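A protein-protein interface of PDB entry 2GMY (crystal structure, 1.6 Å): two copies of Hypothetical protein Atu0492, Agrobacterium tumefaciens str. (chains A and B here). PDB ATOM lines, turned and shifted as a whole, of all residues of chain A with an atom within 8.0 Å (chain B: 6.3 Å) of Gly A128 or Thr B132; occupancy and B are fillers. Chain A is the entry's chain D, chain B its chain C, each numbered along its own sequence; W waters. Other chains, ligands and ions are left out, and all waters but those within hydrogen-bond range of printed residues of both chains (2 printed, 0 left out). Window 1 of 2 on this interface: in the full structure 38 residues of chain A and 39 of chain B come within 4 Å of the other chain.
The backbone carbonyl oxygen (O) of Gly B128 sits at hydrogen-bond distance from the side-chain hydroxyl (OG1) of Thr A132 (3.1 Å). O of Gly A128 sits at hydrogen-bond distance from OG1 of Thr B132 (3.1 Å). NE of Arg B135 sits at hydrogen-bond distance from O of Val A95 (2.8 Å). The backbone carbonyl oxygen (O) of Thr A96 is in hydrogen-bond range of the guanidinium group (NH2) of Arg B135, 2.9 Å away. NH2 of Arg B135 sits close to NH2 of Arg A135 (3.3 Å).
The guanidinium group (NH1) of Arg A135 lies within hydrogen-bond range of the side-chain amide oxygen (OD1) of Asn A131, 2.9 Å away. The side-chain amide nitrogen (ND2) of Asn A46 is in hydrogen-bond range of the side-chain amide oxygen (OD1) of Asn A131, at 3.0 Å. O of Gly B128 lies within hydrogen-bond range of OG1 of Thr B132. OD1 of Asn B131 lies within hydrogen-bond range of NH1 of Arg B135 (2.9 Å). O of Ile A127 lies within hydrogen-bond range of ND2 of Asn A131 (2.8 Å). The backbone carbonyl oxygen of Ile B127 lies within hydrogen-bond range of the side-chain amide nitrogen of Asn B131 (2.9 Å).
Leu A21 touches Leu B21 (CD2 to CD2, 3.9 Å). Ile A98 touches Arg B135 (CG2 to CZ, 3.7 Å). Val A125 touches Val B18 (CG2 to CG2, 3.8 Å). Asn A131 touches Arg B135 (OD1 to NE, 3.96 Å). Thr A132 touches Thr B132. Arg A135 touches Asn B131.
Gly A128 touches just one residue of chain B: Thr B132 (3.1 Å). Thr B132 touches just these residues of chain A: Gly A128 and Thr A132. Printed residues of chain B within 4 Å of Leu A21: Leu B21. Of the printed residues of chain B, Arg A135 touches Asn B131 (3.98 Å) and Arg B135 (3.3 Å). Ile B127 touches none of the printed residues of chain A. The nearest residue of chain B that does not touch Gly A128 is Arg B135 (4.8 Å).
Printed residues of chain B that touch a printed residue of chain A: Val B18, Leu B21, Gly B128, Asn B131, Thr B132 and Arg B135. Hydrophobic or aromatic side chains of chain B that line the printed part of chain A: Val B18 and Leu B21. Hydrophobic or aromatic side chains of chain A within 4 Å of the printed part of chain B: Leu A21, Val A95, Ile A98 and Val A125. Among the printed residues, 11 pairs touch across the chains. Among the printed residues, no Asp or Glu carboxylate lies within 4 Å of a Lys or Arg side-chain nitrogen of the other chain.
Leu A21 touches its own counterpart, Leu B21. Gly A128 touches Thr B132, and with the chains exchanged Thr A132 touches Gly B128. Asn A131 touches Arg B135, and with the chains exchanged Arg A135 touches Asn B131. Thr B132 touches its own counterpart, Thr A132. Positions printed for both chains: 18, 21, 127, 128, 129, 130, 131, 132, 133, 134 and 135. Of the 11 pairs that touch across the chains among the printed residues, 7 have their exchanged pair printed and touching as well.
Water W2 lies within hydrogen-bond range of OG1 of Thr A132 (2.6 Å) and OG1 of Thr B132 (2.7 Å). Water W1 lies within hydrogen-bond range of the backbone carbonyl oxygen (O) of Gly A128 (2.9 Å), the backbone carbonyl oxygen (O) of Gly B128 (2.9 Å), the side-chain hydroxyl (OG1) of Thr B132 (2.9 Å) and the side-chain hydroxyl (OG1) of Thr A132 (2.9 Å).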
ATOM      1  N   VAL A  18       2.483  -1.599  17.324  1.00  0.00           N
ATOM      2  CA  VAL A  18       1.919  -2.946  17.144  1.00  0.00           C
ATOM      3  C   VAL A  18       2.047  -3.763  18.435  1.00  0.00           C
ATOM      4  O   VAL A  18       1.109  -4.444  18.834  1.00  0.00           O
ATOM      5  CB  VAL A  18       2.529  -3.684  15.934  1.00  0.00           C
ATOM      6  CG1 VAL A  18       1.894  -5.062  15.777  1.00  0.00           C
ATOM      7  CG2 VAL A  18       2.290  -2.889  14.661  1.00  0.00           C
ATOM      8  N   LEU A  21      -0.689  -3.067  20.966  1.00  0.00           N
ATOM      9  CA  LEU A  21      -1.895  -3.825  20.670  1.00  0.00           C
ATOM     10  C   LEU A  21      -1.764  -5.280  21.135  1.00  0.00           C
ATOM     11  O   LEU A  21      -2.691  -5.838  21.730  1.00  0.00           O
ATOM     12  CB  LEU A  21      -2.218  -3.778  19.172  1.00  0.00           C
ATOM     13  CG  LEU A  21      -3.527  -4.493  18.803  1.00  0.00           C
ATOM     14  CD1 LEU A  21      -4.715  -4.017  19.638  1.00  0.00           C
ATOM     15  CD2 LEU A  21      -3.799  -4.335  17.298  1.00  0.00           C
ATOM     16  N   GLU A  22      -0.613  -5.885  20.858  1.00  0.00           N
ATOM     17  CA  GLU A  22      -0.291  -7.232  21.339  1.00  0.00           C
ATOM     18  C   GLU A  22      -0.413  -7.342  22.866  1.00  0.00           C
ATOM     19  O   GLU A  22      -1.019  -8.292  23.393  1.00  0.00           O
ATOM     20  CB  GLU A  22       1.130  -7.600  20.892  1.00  0.00           C
ATOM     21  CG  GLU A  22       1.587  -8.977  21.331  1.00  0.00           C
ATOM     22  CD  GLU A  22       0.715 -10.077  20.757  1.00  0.00           C
ATOM     23  OE1 GLU A  22       0.168  -9.894  19.641  1.00  0.00           O
ATOM     24  OE2 GLU A  22       0.580 -11.117  21.440  1.00  0.00           O
ATOM     25  N   VAL A  25      -3.959  -7.446  23.907  1.00  0.00           N
ATOM     26  CA  VAL A  25      -4.514  -8.782  23.676  1.00  0.00           C
ATOM     27  C   VAL A  25      -4.159  -9.719  24.838  1.00  0.00           C
ATOM     28  O   VAL A  25      -5.043 -10.359  25.408  1.00  0.00           O
ATOM     29  CB  VAL A  25      -4.083  -9.371  22.305  1.00  0.00           C
ATOM     30  CG1 VAL A  25      -4.512 -10.844  22.187  1.00  0.00           C
ATOM     31  CG2 VAL A  25      -4.693  -8.549  21.174  1.00  0.00           C
ATOM     32  N   ILE A  38      -6.119 -18.688  18.505  1.00  0.00           N
ATOM     33  CA  ILE A  38      -6.295 -17.628  17.515  1.00  0.00           C
ATOM     34  C   ILE A  38      -4.992 -17.365  16.790  1.00  0.00           C
ATOM     35  O   ILE A  38      -4.954 -17.286  15.563  1.00  0.00           O
ATOM     36  CB  ILE A  38      -6.766 -16.325  18.176  1.00  0.00           C
ATOM     37  CG1 ILE A  38      -8.223 -16.465  18.616  1.00  0.00           C
ATOM     38  CG2 ILE A  38      -6.621 -15.157  17.193  1.00  0.00           C
ATOM     39  CD1 ILE A  38      -8.629 -15.463  19.694  1.00  0.00           C
ATOM     40  N   ALA A  42      -4.519 -18.579  12.784  1.00  0.00           N
ATOM     41  CA  ALA A  42      -4.377 -17.483  11.802  1.00  0.00           C
ATOM     42  C   ALA A  42      -3.014 -17.511  11.112  1.00  0.00           C
ATOM     43  O   ALA A  42      -2.921 -17.311   9.903  1.00  0.00           O
ATOM     44  CB  ALA A  42      -4.619 -16.139  12.453  1.00  0.00           C
ATOM     45  N   ASN A  46      -2.172 -17.874   7.093  1.00  0.00           N
ATOM     46  CA  ASN A  46      -1.408 -16.832   6.421  1.00  0.00           C
ATOM     47  C   ASN A  46      -0.028 -17.250   5.975  1.00  0.00           C
ATOM     48  O   ASN A  46       0.693 -16.448   5.386  1.00  0.00           O
ATOM     49  CB  ASN A  46      -1.333 -15.571   7.289  1.00  0.00           C
ATOM     50  CG  ASN A  46      -2.658 -14.835   7.357  1.00  0.00           C
ATOM     51  OD1 ASN A  46      -3.444 -14.822   6.397  1.00  0.00           O
ATOM     52  ND2 ASN A  46      -2.895 -14.180   8.484  1.00  0.00           N
ATOM     53  N   VAL A  95     -12.740 -14.762   9.485  1.00  0.00           N
ATOM     54  CA  VAL A  95     -12.247 -13.390   9.646  1.00  0.00           C
ATOM     55  C   VAL A  95     -10.840 -13.223   9.078  1.00  0.00           C
ATOM     56  O   VAL A  95     -10.528 -12.178   8.497  1.00  0.00           O
ATOM     57  CB  VAL A  95     -12.315 -12.945  11.126  1.00  0.00           C
ATOM     58  CG1 VAL A  95     -11.752 -11.543  11.312  1.00  0.00           C
ATOM     59  CG2 VAL A  95     -13.761 -12.979  11.626  1.00  0.00           C
ATOM     60  N   THR A  96      -9.984 -14.238   9.242  1.00  0.00           N
ATOM     61  CA  THR A  96      -8.678 -14.198   8.588  1.00  0.00           C
ATOM     62  C   THR A  96      -8.819 -14.086   7.070  1.00  0.00           C
ATOM     63  O   THR A  96      -8.075 -13.347   6.423  1.00  0.00           O
ATOM     64  CB  THR A  96      -7.804 -15.392   8.995  1.00  0.00           C
ATOM     65  OG1 THR A  96      -7.599 -15.346  10.415  1.00  0.00           O
ATOM     66  CG2 THR A  96      -6.452 -15.336   8.283  1.00  0.00           C
ATOM     67  N   ILE A  98     -11.286 -12.681   5.407  1.00  0.00           N
ATOM     68  CA  ILE A  98     -12.461 -11.801   5.317  1.00  0.00           C
ATOM     69  C   ILE A  98     -12.854 -11.419   3.883  1.00  0.00           C
ATOM     70  O   ILE A  98     -14.048 -11.305   3.574  1.00  0.00           O
ATOM     71  CB  ILE A  98     -12.261 -10.518   6.184  1.00  0.00           C
ATOM     72  CG1 ILE A  98     -13.601  -9.822   6.461  1.00  0.00           C
ATOM     73  CG2 ILE A  98     -11.224  -9.574   5.553  1.00  0.00           C
ATOM     74  CD1 ILE A  98     -14.385 -10.434   7.606  1.00  0.00           C
ATOM     75  N   VAL A 121     -15.550  -9.234  20.791  1.00  0.00           N
ATOM     76  CA  VAL A 121     -14.737  -8.092  20.406  1.00  0.00           C
ATOM     77  C   VAL A 121     -13.262  -8.401  20.690  1.00  0.00           C
ATOM     78  O   VAL A 121     -12.407  -8.201  19.832  1.00  0.00           O
ATOM     79  CB  VAL A 121     -15.195  -6.774  21.100  1.00  0.00           C
ATOM     80  CG1 VAL A 121     -14.257  -5.636  20.730  1.00  0.00           C
ATOM     81  CG2 VAL A 121     -16.613  -6.422  20.674  1.00  0.00           C
ATOM     82  N   LYS A 122     -12.970  -8.920  21.883  1.00  0.00           N
ATOM     83  CA  LYS A 122     -11.595  -9.263  22.243  1.00  0.00           C
ATOM     84  C   LYS A 122     -11.025 -10.284  21.256  1.00  0.00           C
ATOM     85  O   LYS A 122      -9.893 -10.131  20.787  1.00  0.00           O
ATOM     86  CB  LYS A 122     -11.521  -9.777  23.675  1.00  0.00           C
ATOM     87  CG  LYS A 122     -11.922  -8.713  24.713  1.00  0.00           C
ATOM     88  CD  LYS A 122     -11.925  -9.290  26.112  1.00  0.00           C
ATOM     89  CE  LYS A 122     -12.352  -8.238  27.134  1.00  0.00           C
ATOM     90  NZ  LYS A 122     -12.463  -8.859  28.482  1.00  0.00           N
ATOM     91  N   ILE A 123     -11.816 -11.312  20.942  1.00  0.00           N
ATOM     92  CA  ILE A 123     -11.408 -12.348  19.974  1.00  0.00           C
ATOM     93  C   ILE A 123     -11.088 -11.732  18.619  1.00  0.00           C
ATOM     94  O   ILE A 123     -10.065 -12.065  18.003  1.00  0.00           O
ATOM     95  CB  ILE A 123     -12.532 -13.416  19.815  1.00  0.00           C
ATOM     96  CG1 ILE A 123     -12.584 -14.311  21.043  1.00  0.00           C
ATOM     97  CG2 ILE A 123     -12.344 -14.256  18.545  1.00  0.00           C
ATOM     98  CD1 ILE A 123     -13.932 -14.989  21.200  1.00  0.00           C
ATOM     99  N   THR A 124     -11.954 -10.834  18.160  1.00  0.00           N
ATOM    100  CA  THR A 124     -11.810 -10.270  16.823  1.00  0.00           C
ATOM    101  C   THR A 124     -10.655  -9.288  16.759  1.00  0.00           C
ATOM    102  O   THR A 124      -9.920  -9.248  15.764  1.00  0.00           O
ATOM    103  CB  THR A 124     -13.125  -9.658  16.345  1.00  0.00           C
ATOM    104  OG1 THR A 124     -14.164 -10.640  16.479  1.00  0.00           O
ATOM    105  CG2 THR A 124     -13.035  -9.253  14.888  1.00  0.00           C
ATOM    106  N   VAL A 125     -10.457  -8.517  17.831  1.00  0.00           N
ATOM    107  CA  VAL A 125      -9.251  -7.691  17.917  1.00  0.00           C
ATOM    108  C   VAL A 125      -7.986  -8.574  17.906  1.00  0.00           C
ATOM    109  O   VAL A 125      -7.008  -8.265  17.199  1.00  0.00           O
ATOM    110  CB  VAL A 125      -9.289  -6.772  19.154  1.00  0.00           C
ATOM    111  CG1 VAL A 125      -7.931  -6.093  19.387  1.00  0.00           C
ATOM    112  CG2 VAL A 125     -10.399  -5.722  18.990  1.00  0.00           C
ATOM    113  N   ALA A 126      -8.010  -9.682  18.653  1.00  0.00           N
ATOM    114  CA  ALA A 126      -6.897 -10.633  18.656  1.00  0.00           C
ATOM    115  C   ALA A 126      -6.614 -11.176  17.246  1.00  0.00           C
ATOM    116  O   ALA A 126      -5.450 -11.275  16.825  1.00  0.00           O
ATOM    117  CB  ALA A 126      -7.174 -11.774  19.644  1.00  0.00           C
ATOM    118  N   ILE A 127      -7.676 -11.494  16.508  1.00  0.00           N
ATOM    119  CA  ILE A 127      -7.522 -11.973  15.126  1.00  0.00           C
ATOM    120  C   ILE A 127      -6.874 -10.874  14.274  1.00  0.00           C
ATOM    121  O   ILE A 127      -5.992 -11.134  13.452  1.00  0.00           O
ATOM    122  CB  ILE A 127      -8.874 -12.389  14.539  1.00  0.00           C
ATOM    123  CG1 ILE A 127      -9.426 -13.616  15.282  1.00  0.00           C
ATOM    124  CG2 ILE A 127      -8.754 -12.672  13.031  1.00  0.00           C
ATOM    125  CD1 ILE A 127     -10.881 -13.894  14.939  1.00  0.00           C
ATOM    126  N   GLY A 128      -7.308  -9.634  14.484  1.00  0.00           N
ATOM    127  CA  GLY A 128      -6.714  -8.505  13.750  1.00  0.00           C
ATOM    128  C   GLY A 128      -5.233  -8.399  14.069  1.00  0.00           C
ATOM    129  O   GLY A 128      -4.402  -8.240  13.169  1.00  0.00           O
ATOM    130  N   ALA A 129      -4.902  -8.499  15.357  1.00  0.00           N
ATOM    131  CA  ALA A 129      -3.514  -8.344  15.810  1.00  0.00           C
ATOM    132  C   ALA A 129      -2.591  -9.382  15.168  1.00  0.00           C
ATOM    133  O   ALA A 129      -1.504  -9.048  14.660  1.00  0.00           O
ATOM    134  CB  ALA A 129      -3.438  -8.438  17.324  1.00  0.00           C
ATOM    135  N   ILE A 130      -3.026 -10.640  15.154  1.00  0.00           N
ATOM    136  CA  ILE A 130      -2.145 -11.692  14.602  1.00  0.00           C
ATOM    137  C   ILE A 130      -2.049 -11.559  13.084  1.00  0.00           C
ATOM    138  O   ILE A 130      -0.979 -11.751  12.476  1.00  0.00           O
ATOM    139  CB  ILE A 130      -2.520 -13.116  15.066  1.00  0.00           C
ATOM    140  CG1 ILE A 130      -1.491 -14.143  14.523  1.00  0.00           C
ATOM    141  CG2 ILE A 130      -3.935 -13.466  14.652  1.00  0.00           C
ATOM    142  CD1 ILE A 130      -0.091 -13.924  15.053  1.00  0.00           C
ATOM    143  N   ASN A 131      -3.153 -11.158  12.473  1.00  0.00           N
ATOM    144  CA  ASN A 131      -3.123 -10.852  11.047  1.00  0.00           C
ATOM    145  C   ASN A 131      -2.132  -9.728  10.685  1.00  0.00           C
ATOM    146  O   ASN A 131      -1.527  -9.746   9.603  1.00  0.00           O
ATOM    147  CB  ASN A 131      -4.535 -10.562  10.569  1.00  0.00           C
ATOM    148  CG  ASN A 131      -5.223 -11.830  10.092  1.00  0.00           C
ATOM    149  OD1 ASN A 131      -5.111 -12.211   8.925  1.00  0.00           O
ATOM    150  ND2 ASN A 131      -5.917 -12.498  10.993  1.00  0.00           N
ATOM    151  N   THR A 132      -1.945  -8.776  11.608  1.00  0.00           N
ATOM    152  CA  THR A 132      -0.949  -7.715  11.417  1.00  0.00           C
ATOM    153  C   THR A 132       0.456  -8.284  11.555  1.00  0.00           C
ATOM    154  O   THR A 132       1.313  -8.050  10.695  1.00  0.00           O
ATOM    155  CB  THR A 132      -1.200  -6.522  12.374  1.00  0.00           C
ATOM    156  OG1 THR A 132      -2.419  -5.883  11.985  1.00  0.00           O
ATOM    157  CG2 THR A 132      -0.057  -5.494  12.319  1.00  0.00           C
ATOM    158  N   TRP A 133       0.711  -9.031  12.624  1.00  0.00           N
ATOM    159  CA  TRP A 133       2.042  -9.638  12.788  1.00  0.00           C
ATOM    160  C   TRP A 133       2.401 -10.542  11.611  1.00  0.00           C
ATOM    161  O   TRP A 133       3.538 -10.543  11.146  1.00  0.00           O
ATOM    162  CB  TRP A 133       2.148 -10.453  14.070  1.00  0.00           C
ATOM    163  CG  TRP A 133       2.217  -9.669  15.320  1.00  0.00           C
ATOM    164  CD1 TRP A 133       1.355  -9.750  16.369  1.00  0.00           C
ATOM    165  CD2 TRP A 133       3.222  -8.710  15.691  1.00  0.00           C
ATOM    166  NE1 TRP A 133       1.754  -8.898  17.378  1.00  0.00           N
ATOM    167  CE2 TRP A 133       2.896  -8.249  16.985  1.00  0.00           C
ATOM    168  CE3 TRP A 133       4.363  -8.203  15.058  1.00  0.00           C
ATOM    169  CZ2 TRP A 133       3.671  -7.292  17.658  1.00  0.00           C
ATOM    170  CZ3 TRP A 133       5.137  -7.248  15.729  1.00  0.00           C
ATOM    171  CH2 TRP A 133       4.780  -6.805  17.009  1.00  0.00           C
ATOM    172  N   ASN A 134       1.443 -11.344  11.147  1.00  0.00           N
ATOM    173  CA  ASN A 134       1.715 -12.231  10.013  1.00  0.00           C
ATOM    174  C   ASN A 134       2.125 -11.446   8.766  1.00  0.00           C
ATOM    175  O   ASN A 134       3.018 -11.852   8.014  1.00  0.00           O
ATOM    176  CB  ASN A 134       0.473 -13.059   9.683  1.00  0.00           C
ATOM    177  CG  ASN A 134       0.103 -14.055  10.775  1.00  0.00           C
ATOM    178  OD1 ASN A 134       0.907 -14.432  11.652  1.00  0.00           O
ATOM    179  ND2 ASN A 134      -1.118 -14.527  10.689  1.00  0.00           N
ATOM    180  N   ARG A 135       1.469 -10.307   8.556  1.00  0.00           N
ATOM    181  CA  ARG A 135       1.770  -9.444   7.419  1.00  0.00           C
ATOM    182  C   ARG A 135       3.155  -8.818   7.550  1.00  0.00           C
ATOM    183  O   ARG A 135       3.898  -8.759   6.575  1.00  0.00           O
ATOM    184  CB  ARG A 135       0.654  -8.410   7.235  1.00  0.00           C
ATOM    185  CG  ARG A 135      -0.548  -9.035   6.532  1.00  0.00           C
ATOM    186  CD  ARG A 135      -1.849  -8.211   6.626  1.00  0.00           C
ATOM    187  NE  ARG A 135      -2.878  -8.853   5.793  1.00  0.00           N
ATOM    188  CZ  ARG A 135      -3.615  -9.894   6.193  1.00  0.00           C
ATOM    189  NH1 ARG A 135      -3.443 -10.392   7.419  1.00  0.00           N
ATOM    190  NH2 ARG A 135      -4.505 -10.458   5.371  1.00  0.00           N
ATOM    191  N   VAL B  18      -7.322  -0.566  19.844  1.00  0.00           N
ATOM    192  CA  VAL B  18      -7.246  -0.433  18.387  1.00  0.00           C
ATOM    193  C   VAL B  18      -7.087   1.040  17.999  1.00  0.00           C
ATOM    194  O   VAL B  18      -6.325   1.366  17.087  1.00  0.00           O
ATOM    195  CB  VAL B  18      -8.444  -1.088  17.653  1.00  0.00           C
ATOM    196  CG1 VAL B  18      -8.283  -0.955  16.140  1.00  0.00           C
ATOM    197  CG2 VAL B  18      -8.564  -2.559  18.027  1.00  0.00           C
ATOM    198  N   LEU B  21      -3.451   2.196  18.143  1.00  0.00           N
ATOM    199  CA  LEU B  21      -2.701   1.861  16.929  1.00  0.00           C
ATOM    200  C   LEU B  21      -3.090   2.805  15.777  1.00  0.00           C
ATOM    201  O   LEU B  21      -2.233   3.275  15.017  1.00  0.00           O
ATOM    202  CB  LEU B  21      -2.917   0.392  16.542  1.00  0.00           C
ATOM    203  CG  LEU B  21      -2.261  -0.070  15.227  1.00  0.00           C
ATOM    204  CD1 LEU B  21      -0.750   0.172  15.231  1.00  0.00           C
ATOM    205  CD2 LEU B  21      -2.558  -1.540  14.906  1.00  0.00           C
ATOM    206  N   ILE B 127      -0.973  -0.938   6.739  1.00  0.00           N
ATOM    207  CA  ILE B 127      -1.734  -2.002   6.063  1.00  0.00           C
ATOM    208  C   ILE B 127      -2.333  -2.966   7.085  1.00  0.00           C
ATOM    209  O   ILE B 127      -3.497  -3.354   6.978  1.00  0.00           O
ATOM    210  CB  ILE B 127      -0.872  -2.762   5.034  1.00  0.00           C
ATOM    211  CG1 ILE B 127      -0.462  -1.819   3.895  1.00  0.00           C
ATOM    212  CG2 ILE B 127      -1.644  -3.975   4.464  1.00  0.00           C
ATOM    213  CD1 ILE B 127       0.703  -2.337   3.030  1.00  0.00           C
ATOM    214  N   GLY B 128      -1.537  -3.334   8.093  1.00  0.00           N
ATOM    215  CA  GLY B 128      -2.039  -4.195   9.179  1.00  0.00           C
ATOM    216  C   GLY B 128      -3.204  -3.547   9.904  1.00  0.00           C
ATOM    217  O   GLY B 128      -4.246  -4.184  10.123  1.00  0.00           O
ATOM    218  N   ALA B 129      -3.051  -2.263  10.228  1.00  0.00           N
ATOM    219  CA  ALA B 129      -4.098  -1.506  10.921  1.00  0.00           C
ATOM    220  C   ALA B 129      -5.435  -1.510  10.175  1.00  0.00           C
ATOM    221  O   ALA B 129      -6.494  -1.803  10.758  1.00  0.00           O
ATOM    222  CB  ALA B 129      -3.636  -0.051  11.184  1.00  0.00           C
ATOM    223  N   ILE B 130      -5.418  -1.171   8.891  1.00  0.00           N
ATOM    224  CA  ILE B 130      -6.692  -1.107   8.171  1.00  0.00           C
ATOM    225  C   ILE B 130      -7.264  -2.520   8.004  1.00  0.00           C
ATOM    226  O   ILE B 130      -8.480  -2.730   8.074  1.00  0.00           O
ATOM    227  CB  ILE B 130      -6.594  -0.335   6.830  1.00  0.00           C
ATOM    228  CG1 ILE B 130      -7.969  -0.249   6.158  1.00  0.00           C
ATOM    229  CG2 ILE B 130      -5.570  -0.984   5.894  1.00  0.00           C
ATOM    230  CD1 ILE B 130      -9.001   0.585   6.935  1.00  0.00           C
ATOM    231  N   ASN B 131      -6.385  -3.500   7.819  1.00  0.00           N
ATOM    232  CA  ASN B 131      -6.844  -4.879   7.776  1.00  0.00           C
ATOM    233  C   ASN B 131      -7.561  -5.319   9.062  1.00  0.00           C
ATOM    234  O   ASN B 131      -8.507  -6.113   9.013  1.00  0.00           O
ATOM    235  CB  ASN B 131      -5.702  -5.814   7.373  1.00  0.00           C
ATOM    236  CG  ASN B 131      -5.639  -5.990   5.882  1.00  0.00           C
ATOM    237  OD1 ASN B 131      -6.309  -6.857   5.326  1.00  0.00           O
ATOM    238  ND2 ASN B 131      -4.855  -5.154   5.214  1.00  0.00           N
ATOM    239  N   THR B 132      -7.123  -4.779  10.200  1.00  0.00           N
ATOM    240  CA  THR B 132      -7.821  -5.007  11.473  1.00  0.00           C
ATOM    241  C   THR B 132      -9.177  -4.296  11.514  1.00  0.00           C
ATOM    242  O   THR B 132     -10.194  -4.922  11.852  1.00  0.00           O
ATOM    243  CB  THR B 132      -6.928  -4.614  12.663  1.00  0.00           C
ATOM    244  OG1 THR B 132      -5.848  -5.560  12.746  1.00  0.00           O
ATOM    245  CG2 THR B 132      -7.732  -4.609  14.001  1.00  0.00           C
ATOM    246  N   TRP B 133      -9.218  -3.012  11.172  1.00  0.00           N
ATOM    247  CA  TRP B 133     -10.501  -2.314  11.114  1.00  0.00           C
ATOM    248  C   TRP B 133     -11.524  -2.977  10.182  1.00  0.00           C
ATOM    249  O   TRP B 133     -12.720  -3.079  10.515  1.00  0.00           O
ATOM    250  CB  TRP B 133     -10.302  -0.865  10.678  1.00  0.00           C
ATOM    251  CG  TRP B 133      -9.740   0.033  11.739  1.00  0.00           C
ATOM    252  CD1 TRP B 133      -8.561   0.714  11.683  1.00  0.00           C
ATOM    253  CD2 TRP B 133     -10.353   0.388  12.994  1.00  0.00           C
ATOM    254  NE1 TRP B 133      -8.388   1.466  12.832  1.00  0.00           N
ATOM    255  CE2 TRP B 133      -9.472   1.278  13.651  1.00  0.00           C
ATOM    256  CE3 TRP B 133     -11.554   0.033  13.626  1.00  0.00           C
ATOM    257  CZ2 TRP B 133      -9.760   1.828  14.916  1.00  0.00           C
ATOM    258  CZ3 TRP B 133     -11.839   0.570  14.886  1.00  0.00           C
ATOM    259  CH2 TRP B 133     -10.942   1.460  15.513  1.00  0.00           C
ATOM    260  N   ASN B 134     -11.063  -3.394   9.002  1.00  0.00           N
ATOM    261  CA  ASN B 134     -11.937  -4.064   8.050  1.00  0.00           C
ATOM    262  C   ASN B 134     -12.511  -5.343   8.633  1.00  0.00           C
ATOM    263  O   ASN B 134     -13.674  -5.669   8.376  1.00  0.00           O
ATOM    264  CB  ASN B 134     -11.208  -4.408   6.746  1.00  0.00           C
ATOM    265  CG  ASN B 134     -10.752  -3.184   5.973  1.00  0.00           C
ATOM    266  OD1 ASN B 134     -11.264  -2.049   6.137  1.00  0.00           O
ATOM    267  ND2 ASN B 134      -9.794  -3.406   5.108  1.00  0.00           N
ATOM    268  N   ARG B 135     -11.687  -6.077   9.390  1.00  0.00           N
ATOM    269  CA  ARG B 135     -12.163  -7.318  10.005  1.00  0.00           C
ATOM    270  C   ARG B 135     -13.207  -7.044  11.087  1.00  0.00           C
ATOM    271  O   ARG B 135     -14.217  -7.759  11.203  1.00  0.00           O
ATOM    272  CB  ARG B 135     -10.985  -8.140  10.509  1.00  0.00           C
ATOM    273  CG  ARG B 135     -10.279  -8.837   9.334  1.00  0.00           C
ATOM    274  CD  ARG B 135      -8.925  -9.477   9.652  1.00  0.00           C
ATOM    275  NE  ARG B 135      -8.514 -10.241   8.468  1.00  0.00           N
ATOM    276  CZ  ARG B 135      -8.014  -9.708   7.350  1.00  0.00           C
ATOM    277  NH1 ARG B 135      -7.819  -8.394   7.245  1.00  0.00           N
ATOM    278  NH2 ARG B 135      -7.710 -10.497   6.322  1.00  0.00           N
ATOM    279  N   ILE B 136     -12.980  -5.987  11.858  1.00  0.00           N
ATOM    280  CA  ILE B 136     -13.929  -5.587  12.892  1.00  0.00           C
ATOM    281  C   ILE B 136     -15.253  -5.111  12.275  1.00  0.00           C
ATOM    282  O   ILE B 136     -16.332  -5.552  12.693  1.00  0.00           O
ATOM    283  CB  ILE B 136     -13.323  -4.483  13.789  1.00  0.00           C
ATOM    284  CG1 ILE B 136     -12.199  -5.066  14.660  1.00  0.00           C
ATOM    285  CG2 ILE B 136     -14.406  -3.832  14.661  1.00  0.00           C
ATOM    286  CD1 ILE B 136     -11.280  -3.979  15.249  1.00  0.00           C
ATOM    287  N   ALA B 137     -15.168  -4.222  11.284  1.00  0.00           N
ATOM    288  CA  ALA B 137     -16.381  -3.613  10.710  1.00  0.00           C
ATOM    289  C   ALA B 137     -17.211  -4.594   9.891  1.00  0.00           C
ATOM    290  O   ALA B 137     -18.442  -4.645  10.032  1.00  0.00           O
ATOM    291  CB  ALA B 137     -16.036  -2.381   9.882  1.00  0.00           C
HETATM  292  O   HOH W   1      -4.676  -7.061  10.502  1.00  0.00           O
HETATM  293  O   HOH W   2      -3.660  -4.587  13.911  1.00  0.00           O
